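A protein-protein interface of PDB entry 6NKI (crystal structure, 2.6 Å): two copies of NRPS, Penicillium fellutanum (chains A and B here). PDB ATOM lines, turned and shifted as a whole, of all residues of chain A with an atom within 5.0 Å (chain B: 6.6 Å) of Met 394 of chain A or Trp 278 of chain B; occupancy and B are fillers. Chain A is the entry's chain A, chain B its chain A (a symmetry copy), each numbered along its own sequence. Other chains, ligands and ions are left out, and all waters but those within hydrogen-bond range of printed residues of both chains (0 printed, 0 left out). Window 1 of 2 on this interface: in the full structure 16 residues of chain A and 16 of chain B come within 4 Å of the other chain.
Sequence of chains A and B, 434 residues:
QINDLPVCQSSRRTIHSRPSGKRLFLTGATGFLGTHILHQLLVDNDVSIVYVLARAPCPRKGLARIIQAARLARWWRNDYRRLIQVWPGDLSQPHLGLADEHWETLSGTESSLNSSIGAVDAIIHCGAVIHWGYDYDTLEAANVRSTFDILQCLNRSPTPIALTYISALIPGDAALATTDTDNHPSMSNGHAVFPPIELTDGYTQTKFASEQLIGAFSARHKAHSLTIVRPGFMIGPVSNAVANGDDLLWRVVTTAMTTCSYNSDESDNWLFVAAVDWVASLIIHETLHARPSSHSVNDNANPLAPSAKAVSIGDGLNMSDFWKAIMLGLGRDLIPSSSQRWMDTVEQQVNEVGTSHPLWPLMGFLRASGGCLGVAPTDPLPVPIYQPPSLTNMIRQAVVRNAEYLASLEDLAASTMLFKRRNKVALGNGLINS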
ATOM      1  N   VAL A 238      19.645  -7.382  21.939  1.00  0.00           N
ATOM      2  CA  VAL A 238      19.204  -8.341  22.941  1.00  0.00           C
ATOM      3  C   VAL A 238      18.388  -7.641  24.018  1.00  0.00           C
ATOM      4  O   VAL A 238      17.415  -8.195  24.545  1.00  0.00           O
ATOM      5  CB  VAL A 238      20.423  -9.064  23.538  1.00  0.00           C
ATOM      6  CG1 VAL A 238      19.952 -10.210  24.434  1.00  0.00           C
ATOM      7  CG2 VAL A 238      21.376  -9.540  22.440  1.00  0.00           C
ATOM      8  N   TRP A 278      25.313  -3.032  17.133  1.00  0.00           N
ATOM      9  CA  TRP A 278      26.726  -3.260  16.753  1.00  0.00           C
ATOM     10  C   TRP A 278      27.048  -2.570  15.428  1.00  0.00           C
ATOM     11  O   TRP A 278      28.115  -1.975  15.349  1.00  0.00           O
ATOM     12  CB  TRP A 278      27.068  -4.754  16.713  1.00  0.00           C
ATOM     13  CG  TRP A 278      26.751  -5.496  17.974  1.00  0.00           C
ATOM     14  CD1 TRP A 278      26.884  -5.039  19.251  1.00  0.00           C
ATOM     15  CD2 TRP A 278      26.255  -6.842  18.083  1.00  0.00           C
ATOM     16  NE1 TRP A 278      26.493  -5.996  20.145  1.00  0.00           N
ATOM     17  CE2 TRP A 278      26.102  -7.116  19.458  1.00  0.00           C
ATOM     18  CE3 TRP A 278      25.918  -7.841  17.163  1.00  0.00           C
ATOM     19  CZ2 TRP A 278      25.622  -8.340  19.924  1.00  0.00           C
ATOM     20  CZ3 TRP A 278      25.456  -9.052  17.628  1.00  0.00           C
ATOM     21  CH2 TRP A 278      25.305  -9.298  18.991  1.00  0.00           C
ATOM     22  N   SER A 390      31.967 -16.078  20.785  1.00  0.00           N
ATOM     23  CA  SER A 390      31.183 -15.141  21.588  1.00  0.00           C
ATOM     24  C   SER A 390      30.206 -14.333  20.735  1.00  0.00           C
ATOM     25  O   SER A 390      29.125 -13.958  21.215  1.00  0.00           O
ATOM     26  CB  SER A 390      32.121 -14.214  22.381  1.00  0.00           C
ATOM     27  OG  SER A 390      32.930 -13.390  21.558  1.00  0.00           O
ATOM     28  N   LEU A 391      30.558 -14.077  19.480  1.00  0.00           N
ATOM     29  CA  LEU A 391      29.691 -13.277  18.625  1.00  0.00           C
ATOM     30  C   LEU A 391      28.572 -14.142  18.084  1.00  0.00           C
ATOM     31  O   LEU A 391      27.402 -13.741  18.116  1.00  0.00           O
ATOM     32  CB  LEU A 391      30.519 -12.622  17.506  1.00  0.00           C
ATOM     33  CG  LEU A 391      29.882 -11.859  16.344  1.00  0.00           C
ATOM     34  CD1 LEU A 391      29.122 -10.645  16.797  1.00  0.00           C
ATOM     35  CD2 LEU A 391      30.930 -11.514  15.326  1.00  0.00           C
ATOM     36  N   THR A 392      28.933 -15.348  17.634  1.00  0.00           N
ATOM     37  CA  THR A 392      27.954 -16.377  17.314  1.00  0.00           C
ATOM     38  C   THR A 392      26.938 -16.499  18.429  1.00  0.00           C
ATOM     39  O   THR A 392      25.731 -16.494  18.173  1.00  0.00           O
ATOM     40  CB  THR A 392      28.662 -17.708  17.082  1.00  0.00           C
ATOM     41  OG1 THR A 392      29.726 -17.537  16.139  1.00  0.00           O
ATOM     42  CG2 THR A 392      27.679 -18.766  16.548  1.00  0.00           C
ATOM     43  N   ASN A 393      27.394 -16.572  19.686  1.00  0.00           N
ATOM     44  CA  ASN A 393      26.425 -16.754  20.762  1.00  0.00           C
ATOM     45  C   ASN A 393      25.542 -15.528  20.947  1.00  0.00           C
ATOM     46  O   ASN A 393      24.355 -15.654  21.270  1.00  0.00           O
ATOM     47  CB  ASN A 393      27.063 -17.037  22.120  1.00  0.00           C
ATOM     48  CG  ASN A 393      26.002 -17.411  23.154  1.00  0.00           C
ATOM     49  OD1 ASN A 393      25.072 -18.166  22.839  1.00  0.00           O
ATOM     50  ND2 ASN A 393      25.967 -16.658  24.248  1.00  0.00           N
ATOM     51  N   MET A 394      26.097 -14.334  20.782  1.00  0.00           N
ATOM     52  CA  MET A 394      25.308 -13.147  21.111  1.00  0.00           C
ATOM     53  C   MET A 394      24.256 -12.842  20.042  1.00  0.00           C
ATOM     54  O   MET A 394      23.204 -12.280  20.373  1.00  0.00           O
ATOM     55  CB  MET A 394      26.201 -11.937  21.310  1.00  0.00           C
ATOM     56  CG  MET A 394      25.538 -10.912  22.213  1.00  0.00           C
ATOM     57  SD  MET A 394      25.425 -11.521  23.929  1.00  0.00           S
ATOM     58  CE  MET A 394      24.196 -10.428  24.654  1.00  0.00           C
ATOM     59  N   ILE A 395      24.513 -13.198  18.778  1.00  0.00           N
ATOM     60  CA  ILE A 395      23.437 -13.099  17.794  1.00  0.00           C
ATOM     61  C   ILE A 395      22.428 -14.220  18.006  1.00  0.00           C
ATOM     62  O   ILE A 395      21.219 -13.968  17.955  1.00  0.00           O
ATOM     63  CB  ILE A 395      23.967 -13.087  16.346  1.00  0.00           C
ATOM     64  CG1 ILE A 395      24.675 -14.372  16.026  1.00  0.00           C
ATOM     65  CG2 ILE A 395      25.008 -12.002  16.093  1.00  0.00           C
ATOM     66  CD1 ILE A 395      25.256 -14.361  14.685  1.00  0.00           C
ATOM     67  N   ARG A 396      22.893 -15.456  18.252  1.00  0.00           N
ATOM     68  CA  ARG A 396      21.984 -16.528  18.652  1.00  0.00           C
ATOM     69  C   ARG A 396      21.012 -16.088  19.729  1.00  0.00           C
ATOM     70  O   ARG A 396      19.811 -16.326  19.602  1.00  0.00           O
ATOM     71  CB  ARG A 396      22.781 -17.770  19.068  1.00  0.00           C
ATOM     72  CG  ARG A 396      22.007 -18.739  19.913  1.00  0.00           C
ATOM     73  CD  ARG A 396      22.652 -20.067  20.124  1.00  0.00           C
ATOM     74  NE  ARG A 396      24.010 -20.005  20.651  1.00  0.00           N
ATOM     75  CZ  ARG A 396      25.092 -20.447  19.999  1.00  0.00           C
ATOM     76  NH1 ARG A 396      24.995 -21.106  18.837  1.00  0.00           N
ATOM     77  NH2 ARG A 396      26.290 -20.246  20.532  1.00  0.00           N
ATOM     78  N   GLN A 397      21.484 -15.406  20.756  1.00  0.00           N
ATOM     79  CA  GLN A 397      20.541 -14.939  21.754  1.00  0.00           C
ATOM     80  C   GLN A 397      19.671 -13.822  21.199  1.00  0.00           C
ATOM     81  O   GLN A 397      18.538 -13.631  21.649  1.00  0.00           O
ATOM     82  CB  GLN A 397      21.277 -14.458  23.025  1.00  0.00           C
ATOM     83  CG  GLN A 397      22.103 -15.489  23.682  1.00  0.00           C
ATOM     84  CD  GLN A 397      21.296 -16.690  24.131  1.00  0.00           C
ATOM     85  OE1 GLN A 397      21.430 -17.766  23.559  1.00  0.00           O
ATOM     86  NE2 GLN A 397      20.472 -16.515  25.176  1.00  0.00           N
ATOM     87  N   ALA A 398      20.164 -13.066  20.227  1.00  0.00           N
ATOM     88  CA  ALA A 398      19.310 -12.021  19.675  1.00  0.00           C
ATOM     89  C   ALA A 398      18.110 -12.629  18.947  1.00  0.00           C
ATOM     90  O   ALA A 398      16.972 -12.168  19.125  1.00  0.00           O
ATOM     91  CB  ALA A 398      20.126 -11.093  18.767  1.00  0.00           C
ATOM     92  N   GLN B  40      22.677 -13.177  34.761  1.00  0.00           N
ATOM     93  CA  GLN B  40      22.032 -13.708  33.571  1.00  0.00           C
ATOM     94  C   GLN B  40      21.308 -15.020  33.840  1.00  0.00           C
ATOM     95  O   GLN B  40      20.338 -15.334  33.144  1.00  0.00           O
ATOM     96  CB  GLN B  40      23.043 -13.854  32.437  1.00  0.00           C
ATOM     97  CG  GLN B  40      23.585 -12.538  31.929  1.00  0.00           C
ATOM     98  CD  GLN B  40      24.600 -12.725  30.826  1.00  0.00           C
ATOM     99  OE1 GLN B  40      24.834 -13.841  30.368  1.00  0.00           O
ATOM    100  NE2 GLN B  40      25.252 -11.638  30.435  1.00  0.00           N
ATOM    101  N   VAL B 238      29.378  -2.219  27.826  1.00  0.00           N
ATOM    102  CA  VAL B 238      29.280  -0.846  27.351  1.00  0.00           C
ATOM    103  C   VAL B 238      28.207  -0.094  28.126  1.00  0.00           C
ATOM    104  O   VAL B 238      28.345   1.100  28.416  1.00  0.00           O
ATOM    105  CB  VAL B 238      28.994  -0.840  25.840  1.00  0.00           C
ATOM    106  CG1 VAL B 238      29.097   0.589  25.305  1.00  0.00           C
ATOM    107  CG2 VAL B 238      29.920  -1.805  25.099  1.00  0.00           C
ATOM    108  N   VAL B 273      40.994  -9.213  25.474  1.00  0.00           N
ATOM    109  CA  VAL B 273      40.008  -8.569  26.332  1.00  0.00           C
ATOM    110  C   VAL B 273      38.612  -8.668  25.687  1.00  0.00           C
ATOM    111  O   VAL B 273      38.465  -8.645  24.456  1.00  0.00           O
ATOM    112  CB  VAL B 273      40.452  -7.110  26.632  1.00  0.00           C
ATOM    113  CG1 VAL B 273      40.559  -6.324  25.356  1.00  0.00           C
ATOM    114  CG2 VAL B 273      39.498  -6.407  27.551  1.00  0.00           C
ATOM    115  N   ALA B 274      37.590  -8.781  26.541  1.00  0.00           N
ATOM    116  CA  ALA B 274      36.222  -9.050  26.110  1.00  0.00           C
ATOM    117  C   ALA B 274      35.239  -8.441  27.098  1.00  0.00           C
ATOM    118  O   ALA B 274      35.537  -8.289  28.282  1.00  0.00           O
ATOM    119  CB  ALA B 274      35.936 -10.548  25.966  1.00  0.00           C
ATOM    120  N   ALA B 275      34.094  -8.029  26.594  1.00  0.00           N
ATOM    121  CA  ALA B 275      33.108  -7.578  27.540  1.00  0.00           C
ATOM    122  C   ALA B 275      32.591  -8.800  28.281  1.00  0.00           C
ATOM    123  O   ALA B 275      32.651  -9.925  27.776  1.00  0.00           O
ATOM    124  CB  ALA B 275      31.974  -6.834  26.849  1.00  0.00           C
ATOM    125  N   VAL B 276      32.297  -8.569  29.558  1.00  0.00           N
ATOM    126  CA  VAL B 276      31.898  -9.630  30.520  1.00  0.00           C
ATOM    127  C   VAL B 276      30.577 -10.275  30.122  1.00  0.00           C
ATOM    128  O   VAL B 276      30.528 -11.497  30.107  1.00  0.00           O
ATOM    129  CB  VAL B 276      31.858  -9.082  31.955  1.00  0.00           C
ATOM    130  CG1 VAL B 276      33.256  -8.880  32.490  1.00  0.00           C
ATOM    131  CG2 VAL B 276      31.062  -7.799  32.047  1.00  0.00           C
ATOM    132  N   ASP B 277      29.594  -9.490  29.697  1.00  0.00           N
ATOM    133  CA  ASP B 277      28.268 -10.070  29.361  1.00  0.00           C
ATOM    134  C   ASP B 277      28.391 -11.075  28.215  1.00  0.00           C
ATOM    135  O   ASP B 277      27.676 -12.063  28.244  1.00  0.00           O
ATOM    136  CB  ASP B 277      27.184  -9.005  29.190  1.00  0.00           C
ATOM    137  CG  ASP B 277      27.439  -8.003  28.079  1.00  0.00           C
ATOM    138  OD1 ASP B 277      28.501  -8.063  27.460  1.00  0.00           O
ATOM    139  OD2 ASP B 277      26.562  -7.174  27.850  1.00  0.00           O
ATOM    140  N   TRP B 278      29.229 -10.807  27.225  1.00  0.00           N
ATOM    141  CA  TRP B 278      29.354 -11.760  26.098  1.00  0.00           C
ATOM    142  C   TRP B 278      29.888 -13.107  26.585  1.00  0.00           C
ATOM    143  O   TRP B 278      29.359 -14.116  26.136  1.00  0.00           O
ATOM    144  CB  TRP B 278      30.211 -11.187  24.963  1.00  0.00           C
ATOM    145  CG  TRP B 278      29.758  -9.853  24.458  1.00  0.00           C
ATOM    146  CD1 TRP B 278      28.472  -9.425  24.310  1.00  0.00           C
ATOM    147  CD2 TRP B 278      30.591  -8.766  24.018  1.00  0.00           C
ATOM    148  NE1 TRP B 278      28.446  -8.147  23.824  1.00  0.00           N
ATOM    149  CE2 TRP B 278      29.732  -7.716  23.634  1.00  0.00           C
ATOM    150  CE3 TRP B 278      31.972  -8.569  23.915  1.00  0.00           C
ATOM    151  CZ2 TRP B 278      30.215  -6.493  23.165  1.00  0.00           C
ATOM    152  CZ3 TRP B 278      32.445  -7.365  23.440  1.00  0.00           C
ATOM    153  CH2 TRP B 278      31.578  -6.339  23.074  1.00  0.00           C
ATOM    154  N   VAL B 279      30.863 -13.124  27.495  1.00  0.00           N
ATOM    155  CA  VAL B 279      31.435 -14.392  27.904  1.00  0.00           C
ATOM    156  C   VAL B 279      30.524 -15.051  28.935  1.00  0.00           C
ATOM    157  O   VAL B 279      30.316 -16.271  28.911  1.00  0.00           O
ATOM    158  CB  VAL B 279      32.863 -14.157  28.420  1.00  0.00           C
ATOM    159  CG1 VAL B 279      33.778 -13.756  27.282  1.00  0.00           C
ATOM    160  CG2 VAL B 279      32.858 -13.044  29.411  1.00  0.00           C
ATOM    161  N   ALA B 280      29.928 -14.238  29.804  1.00  0.00           N
ATOM    162  CA  ALA B 280      28.839 -14.678  30.651  1.00  0.00           C
ATOM    163  C   ALA B 280      27.759 -15.381  29.836  1.00  0.00           C
ATOM    164  O   ALA B 280      27.412 -16.537  30.110  1.00  0.00           O
ATOM    165  CB  ALA B 280      28.258 -13.472  31.394  1.00  0.00           C
ATOM    166  N   SER B 281      27.189 -14.669  28.850  1.00  0.00           N
ATOM    167  CA  SER B 281      26.157 -15.229  27.979  1.00  0.00           C
ATOM    168  C   SER B 281      26.627 -16.539  27.366  1.00  0.00           C
ATOM    169  O   SER B 281      25.881 -17.529  27.307  1.00  0.00           O
ATOM    170  CB  SER B 281      25.788 -14.221  26.869  1.00  0.00           C
ATOM    171  OG  SER B 281      24.763 -14.690  25.972  1.00  0.00           O
ATOM    172  N   LEU B 282      27.879 -16.560  26.902  1.00  0.00           N
ATOM    173  CA  LEU B 282      28.419 -17.759  26.281  1.00  0.00           C
ATOM    174  C   LEU B 282      28.606 -18.899  27.281  1.00  0.00           C
ATOM    175  O   LEU B 282      28.654 -20.050  26.865  1.00  0.00           O
ATOM    176  CB  LEU B 282      29.745 -17.438  25.579  1.00  0.00           C
ATOM    177  CG  LEU B 282      30.481 -18.603  24.901  1.00  0.00           C
ATOM    178  CD1 LEU B 282      29.536 -19.288  23.925  1.00  0.00           C
ATOM    179  CD2 LEU B 282      31.724 -18.163  24.165  1.00  0.00           C
ATOM    180  N   ILE B 283      28.728 -18.611  28.578  1.00  0.00           N
ATOM    181  CA  ILE B 283      28.882 -19.685  29.550  1.00  0.00           C
ATOM    182  C   ILE B 283      27.540 -20.334  29.832  1.00  0.00           C
ATOM    183  O   ILE B 283      27.437 -21.564  29.902  1.00  0.00           O
ATOM    184  CB  ILE B 283      29.557 -19.172  30.842  1.00  0.00           C
ATOM    185  CG1 ILE B 283      31.060 -18.902  30.615  1.00  0.00           C
ATOM    186  CG2 ILE B 283      29.358 -20.169  31.963  1.00  0.00           C
ATOM    187  CD1 ILE B 283      31.684 -17.932  31.600  1.00  0.00           C
ATOM    188  N   ASP B 315      38.860 -12.868  21.762  1.00  0.00           N
ATOM    189  CA  ASP B 315      38.415 -11.486  21.587  1.00  0.00           C
ATOM    190  C   ASP B 315      39.479 -10.479  22.037  1.00  0.00           C
ATOM    191  O   ASP B 315      40.122 -10.642  23.078  1.00  0.00           O
ATOM    192  CB  ASP B 315      37.114 -11.194  22.367  1.00  0.00           C
ATOM    193  CG  ASP B 315      35.868 -11.930  21.826  1.00  0.00           C
ATOM    194  OD1 ASP B 315      35.970 -12.651  20.806  1.00  0.00           O
ATOM    195  OD2 ASP B 315      34.758 -11.653  22.366  1.00  0.00           O
ATOM    196  N   SER B 390      32.847  -5.650  13.509  1.00  0.00           N
ATOM    197  CA  SER B 390      31.835  -5.207  14.466  1.00  0.00           C
ATOM    198  C   SER B 390      32.214  -5.556  15.904  1.00  0.00           C
ATOM    199  O   SER B 390      31.853  -4.823  16.838  1.00  0.00           O
ATOM    200  CB  SER B 390      30.466  -5.802  14.097  1.00  0.00           C
ATOM    201  OG  SER B 390      30.427  -7.218  14.165  1.00  0.00           O
ATOM    202  N   LEU B 391      32.949  -6.646  16.096  1.00  0.00           N
ATOM    203  CA  LEU B 391      33.311  -7.058  17.445  1.00  0.00           C
ATOM    204  C   LEU B 391      34.489  -6.239  17.928  1.00  0.00           C
ATOM    205  O   LEU B 391      34.475  -5.730  19.056  1.00  0.00           O
ATOM    206  CB  LEU B 391      33.598  -8.569  17.472  1.00  0.00           C
ATOM    207  CG  LEU B 391      34.168  -9.282  18.699  1.00  0.00           C
ATOM    208  CD1 LEU B 391      33.252  -9.209  19.887  1.00  0.00           C
ATOM    209  CD2 LEU B 391      34.517 -10.699  18.348  1.00  0.00           C
ATOM    210  N   ASN B 393      34.975  -3.278  17.004  1.00  0.00           N
ATOM    211  CA  ASN B 393      34.467  -1.961  17.376  1.00  0.00           C
ATOM    212  C   ASN B 393      33.776  -1.979  18.732  1.00  0.00           C
ATOM    213  O   ASN B 393      33.860  -1.005  19.490  1.00  0.00           O
ATOM    214  CB  ASN B 393      33.457  -1.392  16.383  1.00  0.00           C
ATOM    215  CG  ASN B 393      33.116   0.058  16.722  1.00  0.00           C
ATOM    216  OD1 ASN B 393      34.013   0.839  17.068  1.00  0.00           O
ATOM    217  ND2 ASN B 393      31.829   0.321  16.922  1.00  0.00           N
ATOM    218  N   MET B 394      33.064  -3.052  19.050  1.00  0.00           N
ATOM    219  CA  MET B 394      32.266  -3.021  20.276  1.00  0.00           C
ATOM    220  C   MET B 394      33.131  -3.181  21.529  1.00  0.00           C
ATOM    221  O   MET B 394      32.765  -2.654  22.587  1.00  0.00           O
ATOM    222  CB  MET B 394      31.192  -4.091  20.255  1.00  0.00           C
ATOM    223  CG  MET B 394      30.024  -3.710  21.146  1.00  0.00           C
ATOM    224  SD  MET B 394      29.096  -2.301  20.450  1.00  0.00           S
ATOM    225  CE  MET B 394      28.145  -1.721  21.860  1.00  0.00           C
ATOM    226  N   ILE B 395      34.262  -3.891  21.434  1.00  0.00           N
ATOM    227  CA  ILE B 395      35.190  -3.877  22.563  1.00  0.00           C
ATOM    228  C   ILE B 395      35.920  -2.541  22.624  1.00  0.00           C
ATOM    229  O   ILE B 395      36.068  -1.979  23.714  1.00  0.00           O
ATOM    230  CB  ILE B 395      36.182  -5.057  22.520  1.00  0.00           C
ATOM    231  CG1 ILE B 395      37.049  -4.982  21.297  1.00  0.00           C
ATOM    232  CG2 ILE B 395      35.498  -6.417  22.423  1.00  0.00           C
ATOM    233  CD1 ILE B 395      37.947  -6.129  21.187  1.00  0.00           C
ATOM    234  N   ALA B 398      34.006  -0.487  24.495  1.00  0.00           N
ATOM    235  CA  ALA B 398      33.985  -0.860  25.906  1.00  0.00           C
ATOM    236  C   ALA B 398      35.169  -0.240  26.649  1.00  0.00           C
ATOM    237  O   ALA B 398      34.999   0.303  27.751  1.00  0.00           O
ATOM    238  CB  ALA B 398      33.947  -2.386  26.050  1.00  0.00           C
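OG of Ser 281 of chain B is in hydrogen-bond range of ND2 of Asn 393 of chain A, at 2.9 Å.
ND2 of Asn 393 of chain A lies close to N of Leu 282 of chain B (3.3 Å).
OD2 of Asp 315 of chain B lies within hydrogen-bond range of OG of Ser 390 of chain A (2.6 Å).
N of Val 273 of chain B is in hydrogen-bond range of O of Asp 315 of chain B.
OD1 of Asn 393 of chain A is in hydrogen-bond range of NE of Arg 396 of chain A (3.0 Å).
OE1 of Gln 40 of chain B is in hydrogen-bond range of N of Ser 281 of chain B, 2.9 Å away.
Among the printed residues, pairs that only touch across the chains: Gln 397 of chain A with Ser 281 of chain B (3.6 Å), Met 394 of chain A with Trp 278 of chain B (3.7 Å), Trp 278 of chain A with Met 394 of chain B (3.7 Å), Met 394 of chain A with Ser 281 of chain B (3.8 Å) and Ser 390 of chain A with Leu 282 of chain B (3.98 Å).
Of chain B, only Trp 278 and Ser 281 come within 4 Å of Met 394 of chain A.
Of chain A, only Met 394 comes within 4 Å of Trp 278 of chain B.
Of the printed residues of chain A, Met 394 of chain B touches Trp 278.
Of the printed residues of chain A, Leu 282 of chain B touches Ser 390 and Asn 393.
The nearest residue of chain A that does not touch Trp 278 of chain B is Ser 390 of chain A (4.4 Å).
The nearest printed residue of chain B that does not touch Trp 278 of chain A is Ser 390 of chain B (4.4 Å).
Hydrophobic or aromatic side chains of chain B that line the printed part of chain A: Trp 278, Leu 282 and Met 394.
Of the 11 printed residues of chain A, 5 touch a printed residue of chain B.
Among the printed residues, 8 pairs touch across the chains.
Among the printed residues, no Asp or Glu carboxylate lies within 4 Å of a Lys or Arg side-chain nitrogen of the other chain.
Trp 278 of chain A touches Met 394 of chain B, and with the chains exchanged Met 394 of chain A touches Trp 278 of chain B.
Positions printed for both chains: 238, 278, 390, 391, 393, 394, 395 and 398.
Of the 8 pairs that touch across the chains among the printed residues, 2 have their exchanged pair printed and touching as well.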
